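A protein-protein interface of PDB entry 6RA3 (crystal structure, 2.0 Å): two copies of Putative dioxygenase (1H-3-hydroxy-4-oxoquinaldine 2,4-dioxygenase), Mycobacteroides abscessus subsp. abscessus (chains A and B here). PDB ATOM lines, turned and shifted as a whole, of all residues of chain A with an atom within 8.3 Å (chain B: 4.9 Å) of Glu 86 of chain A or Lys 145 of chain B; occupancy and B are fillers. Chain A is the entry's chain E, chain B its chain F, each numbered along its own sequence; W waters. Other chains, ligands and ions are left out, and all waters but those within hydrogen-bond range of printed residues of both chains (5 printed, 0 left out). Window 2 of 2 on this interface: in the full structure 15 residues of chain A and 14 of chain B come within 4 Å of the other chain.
NE1 of Trp 144 of chain B is in hydrogen-bond range of OE2 of Glu 86 of chain A, at 2.9 Å. The side-chain carboxylate (OD1) of Asp 149 of chain B lies within hydrogen-bond range of a ring nitrogen (NE2) of His 19 of chain A (2.5 Å). NZ of Lys 145 of chain B lies within hydrogen-bond range of O of Glu 86 of chain A (2.7 Å).
Among the printed residues, merely in contact across the chains: Arg 50 of chain A with Arg 148 of chain B (3.7 Å) and Glu 86 of chain A with Phe 177 of chain B (3.5 Å).
Of chain B, only Trp 144 (2.9 Å), Lys 145 (2.7 Å) and Phe 177 (3.5 Å) come within 4 Å of Glu 86 of chain A. Lys 145 of chain B touches just one residue of chain A: Glu 86 (2.7 Å). Printed residues of chain A within 4 Å of Asp 149 of chain B: His 19. Printed residues of chain A within 4 Å of Trp 144 of chain B: Glu 86. Asp 83 of chain A touches none of the printed residues of chain B. Gly 80 of chain A touches none of the printed residues of chain B. The nearest printed residue of chain A that does not touch Arg 148 of chain B is His 19 of chain A (4.8 Å).
Of the 8 printed residues of chain B, 5 touch a printed residue of chain A. Printed residues of chain B that touch a printed residue of chain A: Trp 144, Lys 145, Arg 148, Asp 149 and Phe 177. Hydrophobic or aromatic side chains of chain B within 4 Å of the printed part of chain A: Trp 144 and Phe 177. Of the 17 printed residues of chain A, 3 touch a printed residue of chain B. Hydrophobic or aromatic side chains of chain A within 4 Å of the printed part of chain B: His 19. Among the printed residues, no Asp or Glu carboxylate lies within 4 Å of a Lys or Arg side-chain nitrogen of the other chain.
No position is printed for both chains. Of the 5 pairs that touch across the chains among the printed residues, none has its exchanged pair printed and touching as well.
Water W1 lies within hydrogen-bond range of OE2 of Glu 86 of chain A (2.5 Å) and NZ of Lys 145 of chain B (3.4 Å). Water W4 lies within hydrogen-bond range of the backbone carbonyl oxygen (O) of Leu 85 of chain A (2.7 Å), the guanidinium group (NH2) of Arg 50 of chain A (2.9 Å) and the guanidinium group (NH1) of Arg 148 of chain B (2.9 Å). Water W5 lies within hydrogen-bond range of OD1 of Asp 149 of chain B (2.7 Å) and NE2 of His 19 of chain A (3.3 Å). Water W2 lies within hydrogen-bond range of NH1 of Arg 50 of chain A, O of Leu 85 of chain A, NH2 of Arg 148 of chain B and O of Glu 86 of chain A. Water W3 lies within hydrogen-bond range of the side-chain carboxylate (OE1) of Glu 86 of chain A, the backbone carbonyl oxygen (O) of Ala 84 of chain A and the backbone NH (N) of Phe 177 of chain B.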
ATOM      1  N   LYS A   5      -5.316 -11.246  10.784  1.00  0.00           N
ATOM      2  CA  LYS A   5      -5.632 -11.811   9.483  1.00  0.00           C
ATOM      3  C   LYS A   5      -4.407 -12.548   8.999  1.00  0.00           C
ATOM      4  O   LYS A   5      -3.277 -12.172   9.328  1.00  0.00           O
ATOM      5  CB  LYS A   5      -6.011 -10.756   8.415  1.00  0.00           C
ATOM      6  CG  LYS A   5      -7.377 -10.098   8.506  1.00  0.00           C
ATOM      7  CD  LYS A   5      -7.512  -9.210   7.314  1.00  0.00           C
ATOM      8  CE  LYS A   5      -8.904  -8.802   7.134  1.00  0.00           C
ATOM      9  NZ  LYS A   5      -9.631  -9.892   6.426  1.00  0.00           N
ATOM     10  N   HIS A  19     -13.281   6.460  11.606  1.00  0.00           N
ATOM     11  CA  HIS A  19     -14.070   6.577  10.397  1.00  0.00           C
ATOM     12  C   HIS A  19     -14.083   8.068  10.123  1.00  0.00           C
ATOM     13  O   HIS A  19     -14.716   8.834  10.859  1.00  0.00           O
ATOM     14  CB  HIS A  19     -15.471   6.018  10.577  1.00  0.00           C
ATOM     15  CG  HIS A  19     -16.256   5.988   9.315  1.00  0.00           C
ATOM     16  ND1 HIS A  19     -17.221   6.926   9.017  1.00  0.00           N
ATOM     17  CD2 HIS A  19     -16.192   5.158   8.248  1.00  0.00           C
ATOM     18  CE1 HIS A  19     -17.733   6.664   7.827  1.00  0.00           C
ATOM     19  NE2 HIS A  19     -17.123   5.598   7.338  1.00  0.00           N
ATOM     20  N   VAL A  24      -5.589   7.186   5.706  1.00  0.00           N
ATOM     21  CA  VAL A  24      -5.575   6.387   6.916  1.00  0.00           C
ATOM     22  C   VAL A  24      -4.197   6.460   7.569  1.00  0.00           C
ATOM     23  O   VAL A  24      -3.173   6.303   6.896  1.00  0.00           O
ATOM     24  CB  VAL A  24      -5.962   4.939   6.561  1.00  0.00           C
ATOM     25  CG1 VAL A  24      -5.787   4.011   7.741  1.00  0.00           C
ATOM     26  CG2 VAL A  24      -7.402   4.928   5.988  1.00  0.00           C
ATOM     27  N   ARG A  50      -9.201   7.628  10.374  1.00  0.00           N
ATOM     28  CA  ARG A  50      -9.147   6.183  10.561  1.00  0.00           C
ATOM     29  C   ARG A  50      -7.705   5.763  10.766  1.00  0.00           C
ATOM     30  O   ARG A  50      -6.814   6.188  10.026  1.00  0.00           O
ATOM     31  CB  ARG A  50      -9.742   5.449   9.346  1.00  0.00           C
ATOM     32  CG  ARG A  50      -9.633   3.936   9.427  1.00  0.00           C
ATOM     33  CD  ARG A  50     -10.252   3.322   8.182  1.00  0.00           C
ATOM     34  NE  ARG A  50     -10.276   1.856   8.237  1.00  0.00           N
ATOM     35  CZ  ARG A  50     -10.554   1.094   7.184  1.00  0.00           C
ATOM     36  NH1 ARG A  50     -10.890   1.650   6.030  1.00  0.00           N
ATOM     37  NH2 ARG A  50     -10.537  -0.210   7.290  1.00  0.00           N
ATOM     38  N   ILE A  79       1.347  -4.137   3.392  1.00  0.00           N
ATOM     39  CA  ILE A  79       0.581  -3.817   2.191  1.00  0.00           C
ATOM     40  C   ILE A  79      -0.547  -4.835   1.985  1.00  0.00           C
ATOM     41  O   ILE A  79      -1.713  -4.464   1.750  1.00  0.00           O
ATOM     42  CB  ILE A  79       1.526  -3.755   0.978  1.00  0.00           C
ATOM     43  CG1 ILE A  79       2.511  -2.582   1.138  1.00  0.00           C
ATOM     44  CG2 ILE A  79       0.745  -3.655  -0.307  1.00  0.00           C
ATOM     45  CD1 ILE A  79       3.682  -2.679   0.208  1.00  0.00           C
ATOM     46  N   GLY A  80      -0.234  -6.121   2.186  1.00  0.00           N
ATOM     47  CA  GLY A  80      -1.240  -7.168   2.033  1.00  0.00           C
ATOM     48  C   GLY A  80      -2.406  -6.982   2.984  1.00  0.00           C
ATOM     49  O   GLY A  80      -3.569  -7.157   2.611  1.00  0.00           O
ATOM     50  N   LEU A  81      -2.112  -6.620   4.226  1.00  0.00           N
ATOM     51  CA  LEU A  81      -3.165  -6.337   5.189  1.00  0.00           C
ATOM     52  C   LEU A  81      -4.036  -5.194   4.712  1.00  0.00           C
ATOM     53  O   LEU A  81      -5.268  -5.277   4.737  1.00  0.00           O
ATOM     54  CB  LEU A  81      -2.560  -6.014   6.565  1.00  0.00           C
ATOM     55  CG  LEU A  81      -3.640  -5.616   7.578  1.00  0.00           C
ATOM     56  CD1 LEU A  81      -4.469  -6.870   7.958  1.00  0.00           C
ATOM     57  CD2 LEU A  81      -3.058  -4.895   8.819  1.00  0.00           C
ATOM     58  N   LEU A  82      -3.416  -4.090   4.323  1.00  0.00           N
ATOM     59  CA  LEU A  82      -4.178  -2.903   3.953  1.00  0.00           C
ATOM     60  C   LEU A  82      -4.961  -3.134   2.663  1.00  0.00           C
ATOM     61  O   LEU A  82      -6.080  -2.624   2.510  1.00  0.00           O
ATOM     62  CB  LEU A  82      -3.240  -1.710   3.807  1.00  0.00           C
ATOM     63  CG  LEU A  82      -2.517  -1.296   5.115  1.00  0.00           C
ATOM     64  CD1 LEU A  82      -1.315  -0.325   4.870  1.00  0.00           C
ATOM     65  CD2 LEU A  82      -3.488  -0.705   6.104  1.00  0.00           C
ATOM     66  N   ASP A  83      -4.426  -3.957   1.768  1.00  0.00           N
ATOM     67  CA  ASP A  83      -5.184  -4.331   0.578  1.00  0.00           C
ATOM     68  C   ASP A  83      -6.393  -5.192   0.940  1.00  0.00           C
ATOM     69  O   ASP A  83      -7.460  -5.021   0.374  1.00  0.00           O
ATOM     70  CB  ASP A  83      -4.279  -5.056  -0.402  1.00  0.00           C
ATOM     71  CG  ASP A  83      -3.322  -4.112  -1.137  1.00  0.00           C
ATOM     72  OD1 ASP A  83      -3.481  -2.879  -0.985  1.00  0.00           O
ATOM     73  OD2 ASP A  83      -2.411  -4.611  -1.849  1.00  0.00           O
ATOM     74  N   ALA A  84      -6.251  -6.083   1.922  1.00  0.00           N
ATOM     75  CA  ALA A  84      -7.359  -6.911   2.355  1.00  0.00           C
ATOM     76  C   ALA A  84      -8.470  -6.068   2.959  1.00  0.00           C
ATOM     77  O   ALA A  84      -9.651  -6.394   2.801  1.00  0.00           O
ATOM     78  CB  ALA A  84      -6.857  -7.951   3.350  1.00  0.00           C
ATOM     79  N   LEU A  85      -8.121  -4.983   3.646  1.00  0.00           N
ATOM     80  CA  LEU A  85      -9.110  -4.057   4.175  1.00  0.00           C
ATOM     81  C   LEU A  85      -9.587  -3.031   3.147  1.00  0.00           C
ATOM     82  O   LEU A  85     -10.524  -2.262   3.435  1.00  0.00           O
ATOM     83  CB  LEU A  85      -8.516  -3.337   5.371  1.00  0.00           C
ATOM     84  CG  LEU A  85      -8.181  -4.221   6.560  1.00  0.00           C
ATOM     85  CD1 LEU A  85      -7.337  -3.460   7.554  1.00  0.00           C
ATOM     86  CD2 LEU A  85      -9.517  -4.691   7.151  1.00  0.00           C
ATOM     87  N   GLU A  86      -8.951  -2.990   1.972  1.00  0.00           N
ATOM     88  CA  GLU A  86      -9.230  -1.983   0.914  1.00  0.00           C
ATOM     89  C   GLU A  86      -9.006  -0.547   1.389  1.00  0.00           C
ATOM     90  O   GLU A  86      -9.699   0.390   0.975  1.00  0.00           O
ATOM     91  CB  GLU A  86     -10.638  -2.151   0.328  1.00  0.00           C
ATOM     92  CG  GLU A  86     -10.640  -3.369  -0.550  1.00  0.00           C
ATOM     93  CD  GLU A  86     -11.923  -3.630  -1.360  1.00  0.00           C
ATOM     94  OE1 GLU A  86     -12.306  -4.821  -1.356  1.00  0.00           O
ATOM     95  OE2 GLU A  86     -12.486  -2.700  -2.025  1.00  0.00           O
ATOM     96  N   VAL A  87      -7.984  -0.366   2.214  1.00  0.00           N
ATOM     97  CA  VAL A  87      -7.489   0.973   2.515  1.00  0.00           C
ATOM     98  C   VAL A  87      -6.894   1.561   1.241  1.00  0.00           C
ATOM     99  O   VAL A  87      -6.135   0.898   0.543  1.00  0.00           O
ATOM    100  CB  VAL A  87      -6.453   0.893   3.652  1.00  0.00           C
ATOM    101  CG1 VAL A  87      -5.730   2.231   3.783  1.00  0.00           C
ATOM    102  CG2 VAL A  87      -7.137   0.483   4.934  1.00  0.00           C
ATOM    103  N   ASP A  88      -7.289   2.772   0.899  1.00  0.00           N
ATOM    104  CA  ASP A  88      -6.699   3.441  -0.247  1.00  0.00           C
ATOM    105  C   ASP A  88      -5.448   4.213   0.194  1.00  0.00           C
ATOM    106  O   ASP A  88      -4.429   3.588   0.480  1.00  0.00           O
ATOM    107  CB  ASP A  88      -7.734   4.341  -0.940  1.00  0.00           C
ATOM    108  CG  ASP A  88      -7.366   4.631  -2.410  1.00  0.00           C
ATOM    109  OD1 ASP A  88      -6.396   4.018  -2.948  1.00  0.00           O
ATOM    110  OD2 ASP A  88      -8.062   5.456  -3.040  1.00  0.00           O
ATOM    111  N   SER A  89      -5.490   5.532   0.259  1.00  0.00           N
ATOM    112  CA  SER A  89      -4.284   6.259   0.622  1.00  0.00           C
ATOM    113  C   SER A  89      -4.067   6.180   2.138  1.00  0.00           C
ATOM    114  O   SER A  89      -5.026   6.159   2.930  1.00  0.00           O
ATOM    115  CB  SER A  89      -4.379   7.704   0.159  1.00  0.00           C
ATOM    116  OG  SER A  89      -5.326   8.387   0.949  1.00  0.00           O
ATOM    117  N   PHE A  90      -2.787   6.120   2.533  1.00  0.00           N
ATOM    118  CA  PHE A  90      -2.441   6.016   3.941  1.00  0.00           C
ATOM    119  C   PHE A  90      -1.071   6.619   4.237  1.00  0.00           C
ATOM    120  O   PHE A  90      -0.209   6.782   3.355  1.00  0.00           O
ATOM    121  CB  PHE A  90      -2.526   4.557   4.401  1.00  0.00           C
ATOM    122  CG  PHE A  90      -1.517   3.634   3.773  1.00  0.00           C
ATOM    123  CD1 PHE A  90      -1.807   2.940   2.610  1.00  0.00           C
ATOM    124  CD2 PHE A  90      -0.319   3.381   4.391  1.00  0.00           C
ATOM    125  CE1 PHE A  90      -0.921   2.083   2.081  1.00  0.00           C
ATOM    126  CE2 PHE A  90       0.581   2.514   3.850  1.00  0.00           C
ATOM    127  CZ  PHE A  90       0.286   1.853   2.704  1.00  0.00           C
ATOM    128  N   ARG A 113      -0.826   6.736  -3.364  1.00  0.00           N
ATOM    129  CA  ARG A 113      -1.232   5.778  -2.346  1.00  0.00           C
ATOM    130  C   ARG A 113      -0.624   6.106  -0.982  1.00  0.00           C
ATOM    131  O   ARG A 113      -1.301   6.001   0.038  1.00  0.00           O
ATOM    132  CB  ARG A 113      -0.805   4.380  -2.796  1.00  0.00           C
ATOM    133  CG  ARG A 113      -1.265   3.205  -1.923  1.00  0.00           C
ATOM    134  CD  ARG A 113      -2.701   2.877  -2.131  1.00  0.00           C
ATOM    135  NE  ARG A 113      -3.208   1.925  -1.135  1.00  0.00           N
ATOM    136  CZ  ARG A 113      -2.997   0.608  -1.166  1.00  0.00           C
ATOM    137  NH1 ARG A 113      -2.349   0.049  -2.171  1.00  0.00           N
ATOM    138  NH2 ARG A 113      -3.500  -0.158  -0.216  1.00  0.00           N
ATOM    139  N   ARG B 143     -18.720   0.750  -5.404  1.00  0.00           N
ATOM    140  CA  ARG B 143     -19.165   1.850  -4.557  1.00  0.00           C
ATOM    141  C   ARG B 143     -19.450   1.393  -3.128  1.00  0.00           C
ATOM    142  O   ARG B 143     -20.154   2.087  -2.393  1.00  0.00           O
ATOM    143  CB  ARG B 143     -20.430   2.533  -5.156  1.00  0.00           C
ATOM    144  CG  ARG B 143     -21.677   1.644  -5.206  1.00  0.00           C
ATOM    145  CD  ARG B 143     -22.875   2.145  -6.136  1.00  0.00           C
ATOM    146  NE  ARG B 143     -24.148   1.499  -5.734  1.00  0.00           N
ATOM    147  CZ  ARG B 143     -25.288   1.463  -6.424  1.00  0.00           C
ATOM    148  NH1 ARG B 143     -25.408   2.038  -7.638  1.00  0.00           N
ATOM    149  NH2 ARG B 143     -26.337   0.834  -5.873  1.00  0.00           N
ATOM    150  N   TRP B 144     -18.900   0.261  -2.678  1.00  0.00           N
ATOM    151  CA  TRP B 144     -19.335  -0.244  -1.375  1.00  0.00           C
ATOM    152  C   TRP B 144     -18.900   0.661  -0.238  1.00  0.00           C
ATOM    153  O   TRP B 144     -19.573   0.727   0.789  1.00  0.00           O
ATOM    154  CB  TRP B 144     -18.807  -1.669  -1.152  1.00  0.00           C
ATOM    155  CG  TRP B 144     -17.352  -1.789  -0.892  1.00  0.00           C
ATOM    156  CD1 TRP B 144     -16.360  -1.920  -1.829  1.00  0.00           C
ATOM    157  CD2 TRP B 144     -16.708  -1.855   0.387  1.00  0.00           C
ATOM    158  NE1 TRP B 144     -15.156  -2.076  -1.217  1.00  0.00           N
ATOM    159  CE2 TRP B 144     -15.335  -2.041   0.145  1.00  0.00           C
ATOM    160  CE3 TRP B 144     -17.163  -1.800   1.711  1.00  0.00           C
ATOM    161  CZ2 TRP B 144     -14.412  -2.109   1.164  1.00  0.00           C
ATOM    162  CZ3 TRP B 144     -16.247  -1.882   2.736  1.00  0.00           C
ATOM    163  CH2 TRP B 144     -14.893  -2.054   2.467  1.00  0.00           C
ATOM    164  N   LYS B 145     -17.774   1.360  -0.389  1.00  0.00           N
ATOM    165  CA  LYS B 145     -17.307   2.188   0.710  1.00  0.00           C
ATOM    166  C   LYS B 145     -18.235   3.361   0.941  1.00  0.00           C
ATOM    167  O   LYS B 145     -18.383   3.827   2.085  1.00  0.00           O
ATOM    168  CB  LYS B 145     -15.880   2.655   0.426  1.00  0.00           C
ATOM    169  CG  LYS B 145     -14.886   1.497   0.435  1.00  0.00           C
ATOM    170  CD  LYS B 145     -13.472   2.027   0.276  1.00  0.00           C
ATOM    171  CE  LYS B 145     -12.592   1.065  -0.410  1.00  0.00           C
ATOM    172  NZ  LYS B 145     -11.286   1.676  -0.765  1.00  0.00           N
ATOM    173  N   GLU B 146     -18.852   3.852  -0.133  1.00  0.00           N
ATOM    174  CA  GLU B 146     -19.952   4.806  -0.009  1.00  0.00           C
ATOM    175  C   GLU B 146     -21.130   4.173   0.700  1.00  0.00           C
ATOM    176  O   GLU B 146     -21.794   4.815   1.527  1.00  0.00           O
ATOM    177  CB  GLU B 146     -20.383   5.286  -1.408  1.00  0.00           C
ATOM    178  CG  GLU B 146     -19.208   5.910  -2.230  1.00  0.00           C
ATOM    179  CD  GLU B 146     -19.567   6.206  -3.672  1.00  0.00           C
ATOM    180  OE1 GLU B 146     -20.759   6.485  -3.950  1.00  0.00           O
ATOM    181  OE2 GLU B 146     -18.642   6.153  -4.523  1.00  0.00           O
ATOM    182  N   GLY B 147     -21.451   2.929   0.344  1.00  0.00           N
ATOM    183  CA  GLY B 147     -22.491   2.214   1.074  1.00  0.00           C
ATOM    184  C   GLY B 147     -22.188   2.139   2.562  1.00  0.00           C
ATOM    185  O   GLY B 147     -23.047   2.406   3.407  1.00  0.00           O
ATOM    186  N   ARG B 148     -20.946   1.776   2.905  1.00  0.00           N
ATOM    187  CA  ARG B 148     -20.562   1.692   4.314  1.00  0.00           C
ATOM    188  C   ARG B 148     -20.664   3.040   5.006  1.00  0.00           C
ATOM    189  O   ARG B 148     -21.113   3.114   6.160  1.00  0.00           O
ATOM    190  CB  ARG B 148     -19.132   1.154   4.446  1.00  0.00           C
ATOM    191  CG  ARG B 148     -18.622   1.198   5.907  1.00  0.00           C
ATOM    192  CD  ARG B 148     -17.317   0.450   5.985  1.00  0.00           C
ATOM    193  NE  ARG B 148     -16.292   1.082   5.150  1.00  0.00           N
ATOM    194  CZ  ARG B 148     -15.063   0.586   5.008  1.00  0.00           C
ATOM    195  NH1 ARG B 148     -14.759  -0.544   5.609  1.00  0.00           N
ATOM    196  NH2 ARG B 148     -14.158   1.206   4.260  1.00  0.00           N
ATOM    197  N   ASP B 149     -20.191   4.111   4.352  1.00  0.00           N
ATOM    198  CA  ASP B 149     -20.322   5.450   4.927  1.00  0.00           C
ATOM    199  C   ASP B 149     -21.797   5.805   5.109  1.00  0.00           C
ATOM    200  O   ASP B 149     -22.179   6.371   6.134  1.00  0.00           O
ATOM    201  CB  ASP B 149     -19.661   6.526   4.048  1.00  0.00           C
ATOM    202  CG  ASP B 149     -18.134   6.424   3.979  1.00  0.00           C
ATOM    203  OD1 ASP B 149     -17.463   5.954   4.921  1.00  0.00           O
ATOM    204  OD2 ASP B 149     -17.588   6.847   2.942  1.00  0.00           O
ATOM    205  N   PHE B 177     -14.757  -5.643   2.338  1.00  0.00           N
ATOM    206  CA  PHE B 177     -15.880  -5.770   1.412  1.00  0.00           C
ATOM    207  C   PHE B 177     -16.707  -7.002   1.753  1.00  0.00           C
ATOM    208  O   PHE B 177     -17.942  -6.945   1.770  1.00  0.00           O
ATOM    209  CB  PHE B 177     -15.397  -5.840  -0.044  1.00  0.00           C
ATOM    210  CG  PHE B 177     -16.511  -6.047  -1.041  1.00  0.00           C
ATOM    211  CD1 PHE B 177     -17.519  -5.103  -1.176  1.00  0.00           C
ATOM    212  CD2 PHE B 177     -16.587  -7.204  -1.779  1.00  0.00           C
ATOM    213  CE1 PHE B 177     -18.559  -5.306  -2.067  1.00  0.00           C
ATOM    214  CE2 PHE B 177     -17.651  -7.423  -2.668  1.00  0.00           C
ATOM    215  CZ  PHE B 177     -18.591  -6.469  -2.839  1.00  0.00           C
HETATM  216  O   HOH W   1     -11.838  -0.665  -3.231  1.00  0.00           O
HETATM  217  O   HOH W   2     -11.362   0.431   3.580  1.00  0.00           O
HETATM  218  O   HOH W   3     -11.969  -5.887   1.187  1.00  0.00           O
HETATM  219  O   HOH W   4     -12.173  -1.853   5.564  1.00  0.00           O
HETATM  220  O   HOH W   5     -15.323   7.603   5.397  1.00  0.00           O
